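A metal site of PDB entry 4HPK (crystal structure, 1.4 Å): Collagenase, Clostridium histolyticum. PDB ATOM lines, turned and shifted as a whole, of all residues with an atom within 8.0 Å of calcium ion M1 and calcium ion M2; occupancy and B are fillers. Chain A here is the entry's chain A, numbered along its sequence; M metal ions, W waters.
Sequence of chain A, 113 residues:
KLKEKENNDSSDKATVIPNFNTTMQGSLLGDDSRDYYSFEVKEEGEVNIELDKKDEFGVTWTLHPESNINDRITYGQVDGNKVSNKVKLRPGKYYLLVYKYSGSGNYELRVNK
O of Arg 34 is bound to calcium ion M2 (2.3 Å).
OD2 of Asp 9 binds calcium ion M2, 2.3 Å away.
The side-chain carboxylate (OD1) of Asp 35 binds calcium ion M2 (2.4 Å).
Calcium ion M2 is bound by the side-chain amide oxygen (OD1) of Asn 8.
The side-chain carboxylate (OD1) of Asp 32 binds calcium ion M2, at 2.4 Å.
Calcium ion M2 is bound by the side-chain carboxylate (OE2) of Glu 6.
OE1 of Glu 6 is bound to calcium ion M2, at 2.6 Å.
Five residues have an atom within 4 Å of calcium ion M1: Glu 4, Glu 6, Ser 27, Asp 32 and Asp 35.
The side-chain carboxylate of Glu 4 lies close to the side-chain amide nitrogen of Asn 8 (2.9 Å).
The backbone carbonyl oxygen (O) of Gln 25 lies within hydrogen-bond range of the backbone NH (N) of Glu 4 (3.0 Å).
The backbone NH (N) of Asp 35 lies within hydrogen-bond range of the backbone carbonyl oxygen (O) of Val 98 (2.8 Å).
N of Asp 9 lies within hydrogen-bond range of OD1 of Asn 7.
The backbone NH (N) of Tyr 36 lies within hydrogen-bond range of the backbone carbonyl oxygen (O) of Asn 8 (2.8 Å).
OH of Tyr 107 sits close to OD2 of Asp 35 (2.6 Å).
OG1 of Thr 15 lies within hydrogen-bond range of ND2 of Asn 8, 3.3 Å away.
Six residues have an atom within 4 Å of calcium ion M2: Glu 6, Asn 8, Asp 9, Asp 32, Arg 34 and Asp 35.
The nearest printed residue that does not touch calcium ion M2 is Glu 4 (4.4 Å).
O of Ser 27 binds calcium ion M1, at 2.4 Å.
OE2 of Glu 6 binds calcium ion M1.
Calcium ion M1 is bound by the side-chain carboxylate (OD2) of Asp 32 (2.4 Å).
Calcium ion M1 is bound by water W1 (2.4 Å).
Calcium ion M1 is bound by OE2 of Glu 4 (2.4 Å).
Calcium ion M1 is bound by OD1 of Asp 35 (2.5 Å).
OE1 of Glu 4 is bound to calcium ion M1.
The side-chain carboxylate (OD2) of Asp 35 is bound to calcium ion M1 (2.6 Å).
Calcium ion M1 has eight donor atoms within binding distance.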
ATOM      1  N   GLU A   4     -21.878  10.109 -28.393  1.00  0.00           N
ATOM      2  CA  GLU A   4     -22.528  11.171 -29.166  1.00  0.00           C
ATOM      3  C   GLU A   4     -21.695  11.576 -30.366  1.00  0.00           C
ATOM      4  O   GLU A   4     -20.478  11.317 -30.408  1.00  0.00           O
ATOM      5  CB  GLU A   4     -22.761  12.387 -28.283  1.00  0.00           C
ATOM      6  CG  GLU A   4     -21.442  12.972 -27.759  1.00  0.00           C
ATOM      7  CD  GLU A   4     -21.587  14.346 -27.124  1.00  0.00           C
ATOM      8  OE1 GLU A   4     -22.411  15.156 -27.598  1.00  0.00           O
ATOM      9  OE2 GLU A   4     -20.840  14.620 -26.172  1.00  0.00           O
ATOM     10  N   LYS A   5     -22.338  12.239 -31.322  1.00  0.00           N
ATOM     11  CA  LYS A   5     -21.667  12.702 -32.529  1.00  0.00           C
ATOM     12  C   LYS A   5     -21.833  14.223 -32.679  1.00  0.00           C
ATOM     13  O   LYS A   5     -22.887  14.695 -33.067  1.00  0.00           O
ATOM     14  CB  LYS A   5     -22.230  11.978 -33.761  1.00  0.00           C
ATOM     15  CG  LYS A   5     -21.983  10.469 -33.770  1.00  0.00           C
ATOM     16  CD  LYS A   5     -22.435   9.830 -35.074  1.00  0.00           C
ATOM     17  CE  LYS A   5     -22.429   8.309 -34.987  1.00  0.00           C
ATOM     18  NZ  LYS A   5     -21.101   7.778 -34.562  1.00  0.00           N
ATOM     19  N   GLU A   6     -20.783  14.983 -32.362  1.00  0.00           N
ATOM     20  CA  GLU A   6     -20.802  16.426 -32.598  1.00  0.00           C
ATOM     21  C   GLU A   6     -20.621  16.708 -34.082  1.00  0.00           C
ATOM     22  O   GLU A   6     -20.013  15.896 -34.774  1.00  0.00           O
ATOM     23  CB  GLU A   6     -19.707  17.141 -31.809  1.00  0.00           C
ATOM     24  CG  GLU A   6     -19.881  17.104 -30.303  1.00  0.00           C
ATOM     25  CD  GLU A   6     -21.006  17.975 -29.773  1.00  0.00           C
ATOM     26  OE1 GLU A   6     -21.573  18.812 -30.510  1.00  0.00           O
ATOM     27  OE2 GLU A   6     -21.316  17.822 -28.578  1.00  0.00           O
ATOM     28  N   ASN A   7     -21.145  17.811 -34.600  1.00  0.00           N
ATOM     29  CA  ASN A   7     -21.995  18.778 -33.889  1.00  0.00           C
ATOM     30  C   ASN A   7     -23.426  18.264 -33.792  1.00  0.00           C
ATOM     31  O   ASN A   7     -24.001  17.841 -34.798  1.00  0.00           O
ATOM     32  CB  ASN A   7     -21.968  20.105 -34.673  1.00  0.00           C
ATOM     33  CG  ASN A   7     -22.661  21.214 -33.944  1.00  0.00           C
ATOM     34  OD1 ASN A   7     -23.855  21.131 -33.649  1.00  0.00           O
ATOM     35  ND2 ASN A   7     -21.938  22.299 -33.691  1.00  0.00           N
ATOM     36  N   ASN A   8     -23.988  18.312 -32.580  1.00  0.00           N
ATOM     37  CA  ASN A   8     -25.366  17.883 -32.318  1.00  0.00           C
ATOM     38  C   ASN A   8     -26.149  18.941 -31.547  1.00  0.00           C
ATOM     39  O   ASN A   8     -27.003  18.645 -30.730  1.00  0.00           O
ATOM     40  CB  ASN A   8     -25.373  16.537 -31.576  1.00  0.00           C
ATOM     41  CG  ASN A   8     -24.646  16.603 -30.249  1.00  0.00           C
ATOM     42  OD1 ASN A   8     -24.285  17.680 -29.790  1.00  0.00           O
ATOM     43  ND2 ASN A   8     -24.388  15.455 -29.654  1.00  0.00           N
ATOM     44  N   ASP A   9     -25.891  20.210 -31.860  1.00  0.00           N
ATOM     45  CA  ASP A   9     -26.401  21.302 -31.037  1.00  0.00           C
ATOM     46  C   ASP A   9     -27.853  21.708 -31.377  1.00  0.00           C
ATOM     47  O   ASP A   9     -28.448  22.537 -30.663  1.00  0.00           O
ATOM     48  CB  ASP A   9     -25.461  22.507 -31.134  1.00  0.00           C
ATOM     49  CG  ASP A   9     -24.083  22.251 -30.491  1.00  0.00           C
ATOM     50  OD1 ASP A   9     -23.285  23.201 -30.512  1.00  0.00           O
ATOM     51  OD2 ASP A   9     -23.785  21.142 -29.980  1.00  0.00           O
ATOM     52  N   SER A  10     -28.421  21.144 -32.434  1.00  0.00           N
ATOM     53  CA  SER A  10     -29.804  21.396 -32.838  1.00  0.00           C
ATOM     54  C   SER A  10     -30.482  20.081 -33.214  1.00  0.00           C
ATOM     55  O   SER A  10     -29.792  19.097 -33.476  1.00  0.00           O
ATOM     56  CB  SER A  10     -29.849  22.377 -34.010  1.00  0.00           C
ATOM     57  OG  SER A  10     -29.079  21.873 -35.081  1.00  0.00           O
ATOM     58  N   LYS A  13     -29.563  18.017 -36.233  1.00  0.00           N
ATOM     59  CA  LYS A  13     -28.243  17.407 -36.111  1.00  0.00           C
ATOM     60  C   LYS A  13     -28.197  16.410 -34.955  1.00  0.00           C
ATOM     61  O   LYS A  13     -27.126  16.047 -34.502  1.00  0.00           O
ATOM     62  CB  LYS A  13     -27.196  18.503 -35.892  1.00  0.00           C
ATOM     63  CG  LYS A  13     -26.944  19.385 -37.130  1.00  0.00           C
ATOM     64  CD  LYS A  13     -26.051  20.580 -36.814  1.00  0.00           C
ATOM     65  CE  LYS A  13     -25.972  21.546 -38.004  1.00  0.00           C
ATOM     66  NZ  LYS A  13     -25.476  22.898 -37.610  1.00  0.00           N
ATOM     67  N   THR A  15     -28.050  13.328 -32.388  1.00  0.00           N
ATOM     68  CA  THR A  15     -27.425  12.011 -32.394  1.00  0.00           C
ATOM     69  C   THR A  15     -28.521  10.960 -32.166  1.00  0.00           C
ATOM     70  O   THR A  15     -29.258  11.035 -31.192  1.00  0.00           O
ATOM     71  CB  THR A  15     -26.372  11.864 -31.295  1.00  0.00           C
ATOM     72  OG1 THR A  15     -25.340  12.855 -31.466  1.00  0.00           O
ATOM     73  CG2 THR A  15     -25.756  10.462 -31.314  1.00  0.00           C
ATOM     74  N   GLN A  25     -22.508   7.766 -24.268  1.00  0.00           N
ATOM     75  CA  GLN A  25     -21.527   8.598 -23.562  1.00  0.00           C
ATOM     76  C   GLN A  25     -21.457   9.979 -24.183  1.00  0.00           C
ATOM     77  O   GLN A  25     -21.453  10.114 -25.394  1.00  0.00           O
ATOM     78  CB  GLN A  25     -20.134   7.965 -23.623  1.00  0.00           C
ATOM     79  CG  GLN A  25     -20.027   6.654 -22.856  1.00  0.00           C
ATOM     80  CD  GLN A  25     -18.596   6.174 -22.707  1.00  0.00           C
ATOM     81  OE1 GLN A  25     -17.829   6.206 -23.669  1.00  0.00           O
ATOM     82  NE2 GLN A  25     -18.239   5.732 -21.508  1.00  0.00           N
ATOM     83  N   GLY A  26     -21.468  11.003 -23.347  1.00  0.00           N
ATOM     84  CA  GLY A  26     -21.353  12.354 -23.849  1.00  0.00           C
ATOM     85  C   GLY A  26     -20.624  13.272 -22.906  1.00  0.00           C
ATOM     86  O   GLY A  26     -20.287  12.919 -21.782  1.00  0.00           O
ATOM     87  N   SER A  27     -20.386  14.481 -23.380  1.00  0.00           N
ATOM     88  CA  SER A  27     -19.761  15.517 -22.564  1.00  0.00           C
ATOM     89  C   SER A  27     -20.328  16.864 -22.928  1.00  0.00           C
ATOM     90  O   SER A  27     -20.723  17.068 -24.069  1.00  0.00           O
ATOM     91  CB  SER A  27     -18.246  15.522 -22.733  1.00  0.00           C
ATOM     92  OG  SER A  27     -17.877  16.027 -23.993  1.00  0.00           O
ATOM     93  N   LEU A  28     -20.369  17.756 -21.925  1.00  0.00           N
ATOM     94  CA  LEU A  28     -20.739  19.158 -22.126  1.00  0.00           C
ATOM     95  C   LEU A  28     -19.656  20.017 -21.481  1.00  0.00           C
ATOM     96  O   LEU A  28     -19.817  20.544 -20.388  1.00  0.00           O
ATOM     97  CB  LEU A  28     -22.105  19.466 -21.494  1.00  0.00           C
ATOM     98  CG  LEU A  28     -23.292  18.807 -22.210  1.00  0.00           C
ATOM     99  CD1 LEU A  28     -24.552  18.923 -21.355  1.00  0.00           C
ATOM    100  CD2 LEU A  28     -23.515  19.388 -23.566  1.00  0.00           C
ATOM    101  N   LEU A  29     -18.531  20.118 -22.187  1.00  0.00           N
ATOM    102  CA  LEU A  29     -17.338  20.810 -21.665  1.00  0.00           C
ATOM    103  C   LEU A  29     -17.235  22.188 -22.293  1.00  0.00           C
ATOM    104  O   LEU A  29     -17.404  22.328 -23.491  1.00  0.00           O
ATOM    105  CB  LEU A  29     -16.070  20.029 -21.991  1.00  0.00           C
ATOM    106  CG  LEU A  29     -16.129  18.543 -21.627  1.00  0.00           C
ATOM    107  CD1 LEU A  29     -14.877  17.839 -22.152  1.00  0.00           C
ATOM    108  CD2 LEU A  29     -16.307  18.325 -20.124  1.00  0.00           C
ATOM    109  N   ASP A  31     -17.800  25.556 -23.979  1.00  0.00           N
ATOM    110  CA  ASP A  31     -18.889  26.150 -24.739  1.00  0.00           C
ATOM    111  C   ASP A  31     -19.752  25.136 -25.486  1.00  0.00           C
ATOM    112  O   ASP A  31     -20.669  25.521 -26.213  1.00  0.00           O
ATOM    113  CB  ASP A  31     -18.407  27.320 -25.633  1.00  0.00           C
ATOM    114  CG  ASP A  31     -17.551  26.869 -26.796  1.00  0.00           C
ATOM    115  OD1 ASP A  31     -17.498  25.674 -27.114  1.00  0.00           O
ATOM    116  OD2 ASP A  31     -16.894  27.766 -27.409  1.00  0.00           O
ATOM    117  N   ASP A  32     -19.519  23.838 -25.277  1.00  0.00           N
ATOM    118  CA  ASP A  32     -20.468  22.827 -25.717  1.00  0.00           C
ATOM    119  C   ASP A  32     -21.508  22.681 -24.626  1.00  0.00           C
ATOM    120  O   ASP A  32     -21.259  22.041 -23.613  1.00  0.00           O
ATOM    121  CB  ASP A  32     -19.756  21.496 -25.987  1.00  0.00           C
ATOM    122  CG  ASP A  32     -20.696  20.409 -26.472  1.00  0.00           C
ATOM    123  OD1 ASP A  32     -21.613  20.709 -27.279  1.00  0.00           O
ATOM    124  OD2 ASP A  32     -20.514  19.220 -26.062  1.00  0.00           O
ATOM    125  N   SER A  33     -22.662  23.317 -24.814  1.00  0.00           N
ATOM    126  CA  SER A  33     -23.660  23.357 -23.742  1.00  0.00           C
ATOM    127  C   SER A  33     -24.943  22.611 -24.042  1.00  0.00           C
ATOM    128  O   SER A  33     -25.794  22.528 -23.156  1.00  0.00           O
ATOM    129  CB  SER A  33     -24.001  24.787 -23.368  1.00  0.00           C
ATOM    130  OG  SER A  33     -24.512  25.419 -24.476  1.00  0.00           O
ATOM    131  N   ARG A  34     -25.066  22.068 -25.249  1.00  0.00           N
ATOM    132  CA  ARG A  34     -26.278  21.369 -25.717  1.00  0.00           C
ATOM    133  C   ARG A  34     -25.865  20.150 -26.526  1.00  0.00           C
ATOM    134  O   ARG A  34     -25.014  20.259 -27.425  1.00  0.00           O
ATOM    135  CB  ARG A  34     -27.092  22.284 -26.631  1.00  0.00           C
ATOM    136  CG  ARG A  34     -27.590  23.529 -25.933  1.00  0.00           C
ATOM    137  CD  ARG A  34     -27.982  24.567 -26.910  1.00  0.00           C
ATOM    138  NE  ARG A  34     -28.992  24.098 -27.858  1.00  0.00           N
ATOM    139  CZ  ARG A  34     -30.305  24.311 -27.744  1.00  0.00           C
ATOM    140  NH1 ARG A  34     -30.818  24.963 -26.694  1.00  0.00           N
ATOM    141  NH2 ARG A  34     -31.108  23.863 -28.702  1.00  0.00           N
ATOM    142  N   ASP A  35     -26.465  19.001 -26.201  1.00  0.00           N
ATOM    143  CA  ASP A  35     -26.313  17.781 -26.988  1.00  0.00           C
ATOM    144  C   ASP A  35     -27.726  17.263 -27.300  1.00  0.00           C
ATOM    145  O   ASP A  35     -28.434  16.838 -26.379  1.00  0.00           O
ATOM    146  CB  ASP A  35     -25.538  16.692 -26.228  1.00  0.00           C
ATOM    147  CG  ASP A  35     -24.071  17.039 -26.015  1.00  0.00           C
ATOM    148  OD1 ASP A  35     -23.518  17.885 -26.737  1.00  0.00           O
ATOM    149  OD2 ASP A  35     -23.445  16.412 -25.132  1.00  0.00           O
ATOM    150  N   TYR A  36     -28.127  17.332 -28.561  1.00  0.00           N
ATOM    151  CA  TYR A  36     -29.436  16.797 -28.995  1.00  0.00           C
ATOM    152  C   TYR A  36     -29.334  15.356 -29.404  1.00  0.00           C
ATOM    153  O   TYR A  36     -28.403  14.966 -30.105  1.00  0.00           O
ATOM    154  CB  TYR A  36     -30.025  17.609 -30.151  1.00  0.00           C
ATOM    155  CG  TYR A  36     -31.337  18.322 -29.838  1.00  0.00           C
ATOM    156  CD1 TYR A  36     -31.464  19.679 -29.989  1.00  0.00           C
ATOM    157  CD2 TYR A  36     -32.435  17.617 -29.388  1.00  0.00           C
ATOM    158  CE1 TYR A  36     -32.646  20.319 -29.701  1.00  0.00           C
ATOM    159  CE2 TYR A  36     -33.623  18.249 -29.100  1.00  0.00           C
ATOM    160  CZ  TYR A  36     -33.723  19.596 -29.257  1.00  0.00           C
ATOM    161  OH  TYR A  36     -34.935  20.209 -28.959  1.00  0.00           O
ATOM    162  N   TYR A  37     -30.313  14.564 -28.942  1.00  0.00           N
ATOM    163  CA  TYR A  37     -30.468  13.173 -29.326  1.00  0.00           C
ATOM    164  C   TYR A  37     -31.893  12.952 -29.853  1.00  0.00           C
ATOM    165  O   TYR A  37     -32.780  13.772 -29.619  1.00  0.00           O
ATOM    166  CB  TYR A  37     -30.294  12.270 -28.106  1.00  0.00           C
ATOM    167  CG  TYR A  37     -28.922  12.332 -27.483  1.00  0.00           C
ATOM    168  CD1 TYR A  37     -28.600  13.281 -26.515  1.00  0.00           C
ATOM    169  CD2 TYR A  37     -27.954  11.433 -27.870  1.00  0.00           C
ATOM    170  CE1 TYR A  37     -27.318  13.298 -25.937  1.00  0.00           C
ATOM    171  CE2 TYR A  37     -26.705  11.451 -27.307  1.00  0.00           C
ATOM    172  CZ  TYR A  37     -26.381  12.384 -26.355  1.00  0.00           C
ATOM    173  OH  TYR A  37     -25.104  12.336 -25.832  1.00  0.00           O
ATOM    174  N   LEU A  97     -33.108  16.848 -25.585  1.00  0.00           N
ATOM    175  CA  LEU A  97     -32.068  17.851 -25.481  1.00  0.00           C
ATOM    176  C   LEU A  97     -31.432  17.722 -24.119  1.00  0.00           C
ATOM    177  O   LEU A  97     -32.097  17.974 -23.121  1.00  0.00           O
ATOM    178  CB  LEU A  97     -32.670  19.256 -25.638  1.00  0.00           C
ATOM    179  CG  LEU A  97     -31.724  20.439 -25.398  1.00  0.00           C
ATOM    180  CD1 LEU A  97     -30.531  20.399 -26.355  1.00  0.00           C
ATOM    181  CD2 LEU A  97     -32.494  21.737 -25.546  1.00  0.00           C
ATOM    182  N   VAL A  98     -30.146  17.357 -24.090  1.00  0.00           N
ATOM    183  CA  VAL A  98     -29.365  17.371 -22.858  1.00  0.00           C
ATOM    184  C   VAL A  98     -28.621  18.696 -22.863  1.00  0.00           C
ATOM    185  O   VAL A  98     -27.940  19.022 -23.846  1.00  0.00           O
ATOM    186  CB  VAL A  98     -28.371  16.193 -22.792  1.00  0.00           C
ATOM    187  CG1 VAL A  98     -27.494  16.296 -21.556  1.00  0.00           C
ATOM    188  CG2 VAL A  98     -29.129  14.849 -22.845  1.00  0.00           C
ATOM    189  N   GLY A 105     -18.945  19.065 -17.629  1.00  0.00           N
ATOM    190  CA  GLY A 105     -18.650  17.697 -17.286  1.00  0.00           C
ATOM    191  C   GLY A 105     -19.116  16.671 -18.284  1.00  0.00           C
ATOM    192  O   GLY A 105     -19.660  16.993 -19.335  1.00  0.00           O
ATOM    193  N   TYR A 107     -21.100  12.781 -18.947  1.00  0.00           N
ATOM    194  CA  TYR A 107     -22.329  12.119 -18.519  1.00  0.00           C
ATOM    195  C   TYR A 107     -22.555  10.850 -19.340  1.00  0.00           C
ATOM    196  O   TYR A 107     -21.950  10.658 -20.394  1.00  0.00           O
ATOM    197  CB  TYR A 107     -23.552  13.054 -18.651  1.00  0.00           C
ATOM    198  CG  TYR A 107     -23.861  13.439 -20.088  1.00  0.00           C
ATOM    199  CD1 TYR A 107     -24.702  12.641 -20.876  1.00  0.00           C
ATOM    200  CD2 TYR A 107     -23.300  14.563 -20.684  1.00  0.00           C
ATOM    201  CE1 TYR A 107     -24.965  12.955 -22.199  1.00  0.00           C
ATOM    202  CE2 TYR A 107     -23.550  14.880 -22.002  1.00  0.00           C
ATOM    203  CZ  TYR A 107     -24.393  14.087 -22.745  1.00  0.00           C
ATOM    204  OH  TYR A 107     -24.660  14.392 -24.054  1.00  0.00           O
HETATM  205 CA    CA M   1     -21.256  16.993 -26.367  1.00  0.00          CA
HETATM  206 CA    CA M   2     -23.170  19.381 -28.551  1.00  0.00          CA
HETATM  207  O   HOH W   1     -18.910  16.656 -26.780  1.00  0.00           O
